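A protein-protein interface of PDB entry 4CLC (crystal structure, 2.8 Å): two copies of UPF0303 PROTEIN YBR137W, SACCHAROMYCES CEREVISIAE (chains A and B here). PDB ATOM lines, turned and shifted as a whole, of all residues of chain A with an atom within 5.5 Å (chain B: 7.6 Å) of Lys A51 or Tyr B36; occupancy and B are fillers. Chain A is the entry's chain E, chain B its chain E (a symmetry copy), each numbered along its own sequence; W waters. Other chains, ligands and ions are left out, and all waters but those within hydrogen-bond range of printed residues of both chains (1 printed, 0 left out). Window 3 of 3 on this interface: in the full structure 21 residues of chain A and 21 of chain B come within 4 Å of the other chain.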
ATOM      1  N   ILE A  46      14.052 -22.739 -24.092  1.00  0.00           N
ATOM      2  CA  ILE A  46      13.085 -23.696 -23.567  1.00  0.00           C
ATOM      3  C   ILE A  46      13.518 -24.149 -22.188  1.00  0.00           C
ATOM      4  O   ILE A  46      12.689 -24.444 -21.330  1.00  0.00           O
ATOM      5  CB  ILE A  46      12.926 -24.918 -24.475  1.00  0.00           C
ATOM      6  CG1 ILE A  46      12.491 -24.496 -25.875  1.00  0.00           C
ATOM      7  CG2 ILE A  46      11.900 -25.890 -23.909  1.00  0.00           C
ATOM      8  CD1 ILE A  46      12.580 -25.614 -26.857  1.00  0.00           C
ATOM      9  N   ARG A  47      14.825 -24.199 -21.974  1.00  0.00           N
ATOM     10  CA  ARG A  47      15.337 -24.602 -20.684  1.00  0.00           C
ATOM     11  C   ARG A  47      14.787 -23.646 -19.632  1.00  0.00           C
ATOM     12  O   ARG A  47      14.068 -24.060 -18.705  1.00  0.00           O
ATOM     13  CB  ARG A  47      16.863 -24.606 -20.685  1.00  0.00           C
ATOM     14  CG  ARG A  47      17.466 -25.265 -19.465  1.00  0.00           C
ATOM     15  CD  ARG A  47      18.966 -25.165 -19.482  1.00  0.00           C
ATOM     16  NE  ARG A  47      19.533 -25.922 -18.376  1.00  0.00           N
ATOM     17  CZ  ARG A  47      19.990 -25.373 -17.257  1.00  0.00           C
ATOM     18  NH1 ARG A  47      19.953 -24.059 -17.115  1.00  0.00           N
ATOM     19  NH2 ARG A  47      20.482 -26.136 -16.285  1.00  0.00           N
ATOM     20  N   ASN A  48      15.084 -22.363 -19.820  1.00  0.00           N
ATOM     21  CA  ASN A  48      14.567 -21.302 -18.967  1.00  0.00           C
ATOM     22  C   ASN A  48      13.046 -21.377 -18.774  1.00  0.00           C
ATOM     23  O   ASN A  48      12.546 -21.298 -17.652  1.00  0.00           O
ATOM     24  CB  ASN A  48      14.958 -19.948 -19.550  1.00  0.00           C
ATOM     25  CG  ASN A  48      15.079 -18.871 -18.491  1.00  0.00           C
ATOM     26  OD1 ASN A  48      14.685 -19.071 -17.338  1.00  0.00           O
ATOM     27  ND2 ASN A  48      15.630 -17.717 -18.872  1.00  0.00           N
ATOM     28  N   ALA A  49      12.322 -21.558 -19.876  1.00  0.00           N
ATOM     29  CA  ALA A  49      10.860 -21.598 -19.855  1.00  0.00           C
ATOM     30  C   ALA A  49      10.324 -22.662 -18.909  1.00  0.00           C
ATOM     31  O   ALA A  49       9.533 -22.368 -18.005  1.00  0.00           O
ATOM     32  CB  ALA A  49      10.319 -21.834 -21.263  1.00  0.00           C
ATOM     33  N   VAL A  50      10.760 -23.898 -19.139  1.00  0.00           N
ATOM     34  CA  VAL A  50      10.359 -25.044 -18.327  1.00  0.00           C
ATOM     35  C   VAL A  50      10.724 -24.856 -16.858  1.00  0.00           C
ATOM     36  O   VAL A  50       9.967 -25.213 -15.947  1.00  0.00           O
ATOM     37  CB  VAL A  50      11.015 -26.329 -18.844  1.00  0.00           C
ATOM     38  CG1 VAL A  50      10.783 -27.480 -17.864  1.00  0.00           C
ATOM     39  CG2 VAL A  50      10.484 -26.668 -20.227  1.00  0.00           C
ATOM     40  N   LYS A  51      11.898 -24.282 -16.636  1.00  0.00           N
ATOM     41  CA  LYS A  51      12.348 -24.040 -15.283  1.00  0.00           C
ATOM     42  C   LYS A  51      11.464 -22.998 -14.567  1.00  0.00           C
ATOM     43  O   LYS A  51      11.104 -23.181 -13.401  1.00  0.00           O
ATOM     44  CB  LYS A  51      13.809 -23.620 -15.308  1.00  0.00           C
ATOM     45  CG  LYS A  51      14.590 -24.325 -14.254  1.00  0.00           C
ATOM     46  CD  LYS A  51      16.072 -24.161 -14.411  1.00  0.00           C
ATOM     47  CE  LYS A  51      16.726 -24.841 -13.227  1.00  0.00           C
ATOM     48  NZ  LYS A  51      15.923 -26.039 -12.796  1.00  0.00           N
ATOM     49  N   GLU A  52      11.079 -21.936 -15.282  1.00  0.00           N
ATOM     50  CA  GLU A  52      10.153 -20.932 -14.747  1.00  0.00           C
ATOM     51  C   GLU A  52       8.703 -21.447 -14.556  1.00  0.00           C
ATOM     52  O   GLU A  52       8.006 -21.022 -13.636  1.00  0.00           O
ATOM     53  CB  GLU A  52      10.156 -19.693 -15.641  1.00  0.00           C
ATOM     54  N   ASN A  53       8.229 -22.333 -15.428  1.00  0.00           N
ATOM     55  CA  ASN A  53       6.881 -22.880 -15.261  1.00  0.00           C
ATOM     56  C   ASN A  53       6.792 -24.209 -14.507  1.00  0.00           C
ATOM     57  O   ASN A  53       5.694 -24.639 -14.150  1.00  0.00           O
ATOM     58  CB  ASN A  53       6.213 -23.059 -16.632  1.00  0.00           C
ATOM     59  CG  ASN A  53       5.826 -21.735 -17.271  1.00  0.00           C
ATOM     60  OD1 ASN A  53       4.719 -21.228 -17.056  1.00  0.00           O
ATOM     61  ND2 ASN A  53       6.739 -21.165 -18.062  1.00  0.00           N
ATOM     62  N   PHE A  54       7.924 -24.878 -14.294  1.00  0.00           N
ATOM     63  CA  PHE A  54       7.933 -26.177 -13.603  1.00  0.00           C
ATOM     64  C   PHE A  54       9.187 -26.324 -12.752  1.00  0.00           C
ATOM     65  O   PHE A  54      10.097 -27.082 -13.097  1.00  0.00           O
ATOM     66  CB  PHE A  54       7.852 -27.331 -14.592  1.00  0.00           C
ATOM     67  CG  PHE A  54       6.603 -27.348 -15.409  1.00  0.00           C
ATOM     68  CD1 PHE A  54       6.533 -26.652 -16.606  1.00  0.00           C
ATOM     69  CD2 PHE A  54       5.509 -28.083 -15.000  1.00  0.00           C
ATOM     70  CE1 PHE A  54       5.390 -26.678 -17.372  1.00  0.00           C
ATOM     71  CE2 PHE A  54       4.355 -28.118 -15.762  1.00  0.00           C
ATOM     72  CZ  PHE A  54       4.293 -27.414 -16.951  1.00  0.00           C
ATOM     73  N   PRO A  55       9.226 -25.608 -11.626  1.00  0.00           N
ATOM     74  CA  PRO A  55      10.491 -25.316 -10.940  1.00  0.00           C
ATOM     75  C   PRO A  55      11.198 -26.537 -10.344  1.00  0.00           C
ATOM     76  O   PRO A  55      12.428 -26.600 -10.429  1.00  0.00           O
ATOM     77  CB  PRO A  55      10.067 -24.336  -9.844  1.00  0.00           C
ATOM     78  CG  PRO A  55       8.609 -24.655  -9.591  1.00  0.00           C
ATOM     79  CD  PRO A  55       8.041 -25.134 -10.887  1.00  0.00           C
ATOM     80  N   VAL A  75      19.276 -31.036 -19.098  1.00  0.00           N
ATOM     81  CA  VAL A  75      18.335 -31.360 -18.036  1.00  0.00           C
ATOM     82  C   VAL A  75      18.101 -30.109 -17.198  1.00  0.00           C
ATOM     83  O   VAL A  75      19.005 -29.290 -17.023  1.00  0.00           O
ATOM     84  CB  VAL A  75      18.837 -32.529 -17.160  1.00  0.00           C
ATOM     85  CG1 VAL A  75      18.837 -33.805 -17.977  1.00  0.00           C
ATOM     86  CG2 VAL A  75      20.217 -32.237 -16.610  1.00  0.00           C
ATOM     87  N   THR A  76      16.875 -29.956 -16.705  1.00  0.00           N
ATOM     88  CA  THR A  76      16.434 -28.728 -16.031  1.00  0.00           C
ATOM     89  C   THR A  76      16.736 -28.731 -14.547  1.00  0.00           C
ATOM     90  O   THR A  76      17.324 -27.802 -14.033  1.00  0.00           O
ATOM     91  CB  THR A  76      14.943 -28.474 -16.217  1.00  0.00           C
ATOM     92  OG1 THR A  76      14.229 -29.702 -16.034  1.00  0.00           O
ATOM     93  CG2 THR A  76      14.691 -27.939 -17.599  1.00  0.00           C
ATOM     94  N   TYR A  77      16.226 -29.726 -13.845  1.00  0.00           N
ATOM     95  CA  TYR A  77      16.419 -29.808 -12.410  1.00  0.00           C
ATOM     96  C   TYR A  77      17.239 -31.060 -12.097  1.00  0.00           C
ATOM     97  O   TYR A  77      17.717 -31.729 -13.008  1.00  0.00           O
ATOM     98  CB  TYR A  77      15.061 -29.819 -11.700  1.00  0.00           C
ATOM     99  CG  TYR A  77      15.087 -29.264 -10.299  1.00  0.00           C
ATOM    100  CD1 TYR A  77      15.788 -28.106 -10.005  1.00  0.00           C
ATOM    101  CD2 TYR A  77      14.401 -29.896  -9.273  1.00  0.00           C
ATOM    102  CE1 TYR A  77      15.809 -27.596  -8.724  1.00  0.00           C
ATOM    103  CE2 TYR A  77      14.416 -29.396  -7.994  1.00  0.00           C
ATOM    104  CZ  TYR A  77      15.120 -28.249  -7.721  1.00  0.00           C
ATOM    105  OH  TYR A  77      15.133 -27.752  -6.441  1.00  0.00           O
ATOM    106  N   GLY A  78      17.397 -31.374 -10.817  1.00  0.00           N
ATOM    107  CA  GLY A  78      18.276 -32.443 -10.399  1.00  0.00           C
ATOM    108  C   GLY A  78      17.809 -33.892 -10.427  1.00  0.00           C
ATOM    109  O   GLY A  78      18.605 -34.792 -10.141  1.00  0.00           O
ATOM    110  N   THR B  33      30.811 -30.365  -5.074  1.00  0.00           N
ATOM    111  CA  THR B  33      29.450 -30.103  -5.600  1.00  0.00           C
ATOM    112  C   THR B  33      29.226 -30.310  -7.134  1.00  0.00           C
ATOM    113  O   THR B  33      29.422 -29.401  -7.929  1.00  0.00           O
ATOM    114  CB  THR B  33      28.889 -28.674  -5.162  1.00  0.00           C
ATOM    115  OG1 THR B  33      27.474 -28.624  -5.396  1.00  0.00           O
ATOM    116  CG2 THR B  33      29.548 -27.452  -5.829  1.00  0.00           C
ATOM    117  N   PHE B  34      28.936 -31.530  -7.573  1.00  0.00           N
ATOM    118  CA  PHE B  34      28.398 -31.708  -8.944  1.00  0.00           C
ATOM    119  C   PHE B  34      26.852 -31.814  -9.042  1.00  0.00           C
ATOM    120  O   PHE B  34      26.267 -32.832  -8.657  1.00  0.00           O
ATOM    121  CB  PHE B  34      29.017 -32.961  -9.568  1.00  0.00           C
ATOM    122  CG  PHE B  34      28.850 -33.063 -11.058  1.00  0.00           C
ATOM    123  CD1 PHE B  34      29.670 -32.344 -11.909  1.00  0.00           C
ATOM    124  CD2 PHE B  34      27.904 -33.909 -11.605  1.00  0.00           C
ATOM    125  CE1 PHE B  34      29.529 -32.454 -13.286  1.00  0.00           C
ATOM    126  CE2 PHE B  34      27.758 -34.021 -12.978  1.00  0.00           C
ATOM    127  CZ  PHE B  34      28.570 -33.294 -13.822  1.00  0.00           C
ATOM    128  N   THR B  35      26.199 -30.787  -9.595  1.00  0.00           N
ATOM    129  CA  THR B  35      24.730 -30.800  -9.798  1.00  0.00           C
ATOM    130  C   THR B  35      24.318 -30.622 -11.258  1.00  0.00           C
ATOM    131  O   THR B  35      25.178 -30.481 -12.133  1.00  0.00           O
ATOM    132  CB  THR B  35      24.029 -29.678  -9.028  1.00  0.00           C
ATOM    133  OG1 THR B  35      24.336 -28.425  -9.655  1.00  0.00           O
ATOM    134  CG2 THR B  35      24.453 -29.665  -7.570  1.00  0.00           C
ATOM    135  N   TYR B  36      23.005 -30.589 -11.512  1.00  0.00           N
ATOM    136  CA  TYR B  36      22.496 -30.340 -12.869  1.00  0.00           C
ATOM    137  C   TYR B  36      22.990 -28.990 -13.352  1.00  0.00           C
ATOM    138  O   TYR B  36      23.255 -28.792 -14.536  1.00  0.00           O
ATOM    139  CB  TYR B  36      20.957 -30.372 -12.926  1.00  0.00           C
ATOM    140  CG  TYR B  36      20.300 -29.118 -12.367  1.00  0.00           C
ATOM    141  CD1 TYR B  36      20.142 -27.975 -13.153  1.00  0.00           C
ATOM    142  CD2 TYR B  36      19.856 -29.069 -11.047  1.00  0.00           C
ATOM    143  CE1 TYR B  36      19.581 -26.817 -12.632  1.00  0.00           C
ATOM    144  CE2 TYR B  36      19.276 -27.917 -10.527  1.00  0.00           C
ATOM    145  CZ  TYR B  36      19.139 -26.795 -11.328  1.00  0.00           C
ATOM    146  OH  TYR B  36      18.566 -25.647 -10.828  1.00  0.00           O
ATOM    147  N   GLN B  37      23.093 -28.056 -12.416  1.00  0.00           N
ATOM    148  CA  GLN B  37      23.381 -26.674 -12.746  1.00  0.00           C
ATOM    149  C   GLN B  37      24.861 -26.494 -12.989  1.00  0.00           C
ATOM    150  O   GLN B  37      25.262 -25.667 -13.801  1.00  0.00           O
ATOM    151  CB  GLN B  37      22.900 -25.740 -11.635  1.00  0.00           C
ATOM    152  CG  GLN B  37      22.966 -24.269 -12.005  1.00  0.00           C
ATOM    153  CD  GLN B  37      22.361 -23.968 -13.382  1.00  0.00           C
ATOM    154  OE1 GLN B  37      21.175 -24.235 -13.641  1.00  0.00           O
ATOM    155  NE2 GLN B  37      23.179 -23.396 -14.267  1.00  0.00           N
ATOM    156  N   ASP B  38      25.676 -27.269 -12.284  1.00  0.00           N
ATOM    157  CA  ASP B  38      27.112 -27.217 -12.527  1.00  0.00           C
ATOM    158  C   ASP B  38      27.428 -27.769 -13.914  1.00  0.00           C
ATOM    159  O   ASP B  38      28.283 -27.251 -14.624  1.00  0.00           O
ATOM    160  CB  ASP B  38      27.880 -27.982 -11.443  1.00  0.00           C
ATOM    161  CG  ASP B  38      28.230 -27.106 -10.257  1.00  0.00           C
ATOM    162  OD1 ASP B  38      27.385 -26.281  -9.833  1.00  0.00           O
ATOM    163  OD2 ASP B  38      29.371 -27.211  -9.767  1.00  0.00           O
ATOM    164  N   ALA B  39      26.712 -28.817 -14.292  1.00  0.00           N
ATOM    165  CA  ALA B  39      26.835 -29.398 -15.618  1.00  0.00           C
ATOM    166  C   ALA B  39      26.562 -28.356 -16.686  1.00  0.00           C
ATOM    167  O   ALA B  39      27.343 -28.191 -17.622  1.00  0.00           O
ATOM    168  CB  ALA B  39      25.884 -30.567 -15.769  1.00  0.00           C
ATOM    169  N   PHE B  40      25.452 -27.646 -16.542  1.00  0.00           N
ATOM    170  CA  PHE B  40      25.081 -26.658 -17.539  1.00  0.00           C
ATOM    171  C   PHE B  40      26.025 -25.474 -17.534  1.00  0.00           C
ATOM    172  O   PHE B  40      26.337 -24.947 -18.598  1.00  0.00           O
ATOM    173  CB  PHE B  40      23.654 -26.176 -17.326  1.00  0.00           C
ATOM    174  CG  PHE B  40      23.184 -25.236 -18.387  1.00  0.00           C
ATOM    175  CD1 PHE B  40      22.921 -25.701 -19.671  1.00  0.00           C
ATOM    176  CD2 PHE B  40      23.026 -23.889 -18.117  1.00  0.00           C
ATOM    177  CE1 PHE B  40      22.509 -24.842 -20.661  1.00  0.00           C
ATOM    178  CE2 PHE B  40      22.608 -23.023 -19.105  1.00  0.00           C
ATOM    179  CZ  PHE B  40      22.347 -23.500 -20.382  1.00  0.00           C
ATOM    180  N   ASP B  41      26.480 -25.054 -16.349  1.00  0.00           N
ATOM    181  CA  ASP B  41      27.445 -23.953 -16.257  1.00  0.00           C
ATOM    182  C   ASP B  41      28.726 -24.372 -16.942  1.00  0.00           C
ATOM    183  O   ASP B  41      29.285 -23.627 -17.740  1.00  0.00           O
ATOM    184  CB  ASP B  41      27.739 -23.554 -14.807  1.00  0.00           C
ATOM    185  CG  ASP B  41      26.552 -22.883 -14.127  1.00  0.00           C
ATOM    186  OD1 ASP B  41      25.778 -22.196 -14.832  1.00  0.00           O
ATOM    187  OD2 ASP B  41      26.400 -23.029 -12.887  1.00  0.00           O
ATOM    188  N   LEU B  42      29.182 -25.581 -16.643  1.00  0.00           N
ATOM    189  CA  LEU B  42      30.431 -26.066 -17.209  1.00  0.00           C
ATOM    190  C   LEU B  42      30.326 -26.156 -18.735  1.00  0.00           C
ATOM    191  O   LEU B  42      31.251 -25.773 -19.445  1.00  0.00           O
ATOM    192  CB  LEU B  42      30.817 -27.426 -16.604  1.00  0.00           C
ATOM    193  CG  LEU B  42      32.023 -28.149 -17.222  1.00  0.00           C
ATOM    194  CD1 LEU B  42      33.275 -27.275 -17.205  1.00  0.00           C
ATOM    195  CD2 LEU B  42      32.289 -29.459 -16.513  1.00  0.00           C
ATOM    196  N   LEU B  71      23.859 -35.147 -19.643  1.00  0.00           N
ATOM    197  CA  LEU B  71      23.460 -33.869 -19.050  1.00  0.00           C
ATOM    198  C   LEU B  71      23.552 -32.694 -20.031  1.00  0.00           C
ATOM    199  O   LEU B  71      22.693 -31.811 -20.084  1.00  0.00           O
ATOM    200  CB  LEU B  71      24.288 -33.588 -17.791  1.00  0.00           C
ATOM    201  CG  LEU B  71      24.224 -34.749 -16.777  1.00  0.00           C
ATOM    202  CD1 LEU B  71      25.051 -34.467 -15.545  1.00  0.00           C
ATOM    203  CD2 LEU B  71      22.808 -35.094 -16.396  1.00  0.00           C
ATOM    204  N   PHE B  72      24.614 -32.672 -20.813  1.00  0.00           N
ATOM    205  CA  PHE B  72      24.850 -31.522 -21.650  1.00  0.00           C
ATOM    206  C   PHE B  72      25.417 -31.946 -22.978  1.00  0.00           C
ATOM    207  O   PHE B  72      26.356 -32.738 -23.038  1.00  0.00           O
ATOM    208  CB  PHE B  72      25.801 -30.553 -20.957  1.00  0.00           C
ATOM    209  CG  PHE B  72      26.090 -29.317 -21.755  1.00  0.00           C
ATOM    210  CD1 PHE B  72      25.301 -28.188 -21.613  1.00  0.00           C
ATOM    211  CD2 PHE B  72      27.163 -29.275 -22.632  1.00  0.00           C
ATOM    212  CE1 PHE B  72      25.564 -27.045 -22.341  1.00  0.00           C
ATOM    213  CE2 PHE B  72      27.432 -28.137 -23.364  1.00  0.00           C
ATOM    214  CZ  PHE B  72      26.627 -27.015 -23.222  1.00  0.00           C
HETATM  215  O   HOH W   1      21.685 -28.879 -16.960  1.00  0.00           O
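OE1 of Gln B37 lies within hydrogen-bond range of NH2 of Arg A47 (3.3 Å).
NZ of Lys A51 lies close to OH of Tyr B36, 3.3 Å away.
The backbone carbonyl oxygen (O) of Thr A76 sits at hydrogen-bond distance from the side-chain amino group (NZ) of Lys A51 (2.6 Å).
OG1 of Thr B35 is in hydrogen-bond range of N of Gln B37 (3.1 Å).
The side-chain amide nitrogen (NE2) of Gln B37 sits at hydrogen-bond distance from the side-chain carboxylate (OD1) of Asp B41 (2.9 Å).
Among the printed residues, merely in contact across the chains: Arg A47 with Tyr B36 (3.6 Å), Arg A47 with Phe B40 (3.2 Å), Val A75 with Leu B71 (3.6 Å), Thr A76 with Tyr B36 (2.8 Å), Tyr A77 with Tyr B36 (3.5 Å) and Gly A78 with Tyr B36 (3.4 Å).
Lys A51 touches just one residue of chain B: Tyr B36.
Printed residues of chain A within 4 Å of Tyr B36: Arg A47, Lys A51, Thr A76, Tyr A77 and Gly A78.
Of the printed residues of chain B, Val A75 touches Leu B71 (3.6 Å).
Printed residues of chain A within 4 Å of Gln B37: Arg A47.
Of the printed residues of chain B, Arg A47 touches Tyr B36 (3.6 Å), Gln B37 (3.3 Å) and Phe B40 (3.2 Å).
Printed residues of chain A within 4 Å of Leu B71: Val A75 (3.6 Å).
Asn A53 touches none of the printed residues of chain B.
Hydrophobic or aromatic side chains of chain B that line the printed part of chain A: Tyr B36, Phe B40 and Leu B71.
Hydrophobic or aromatic side chains of chain A within 4 Å of the printed part of chain B: Val A75 and Tyr A77.
Among the printed residues, 8 pairs touch across the chains.
No position is printed for both chains.
Of the 8 pairs that touch across the chains among the printed residues, none has its exchanged pair printed and touching as well.
Water W1 lies within hydrogen-bond range of O of Val A75 (2.7 Å), O of Tyr B36 (2.9 Å) and NH2 of Arg A47 (3.1 Å).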
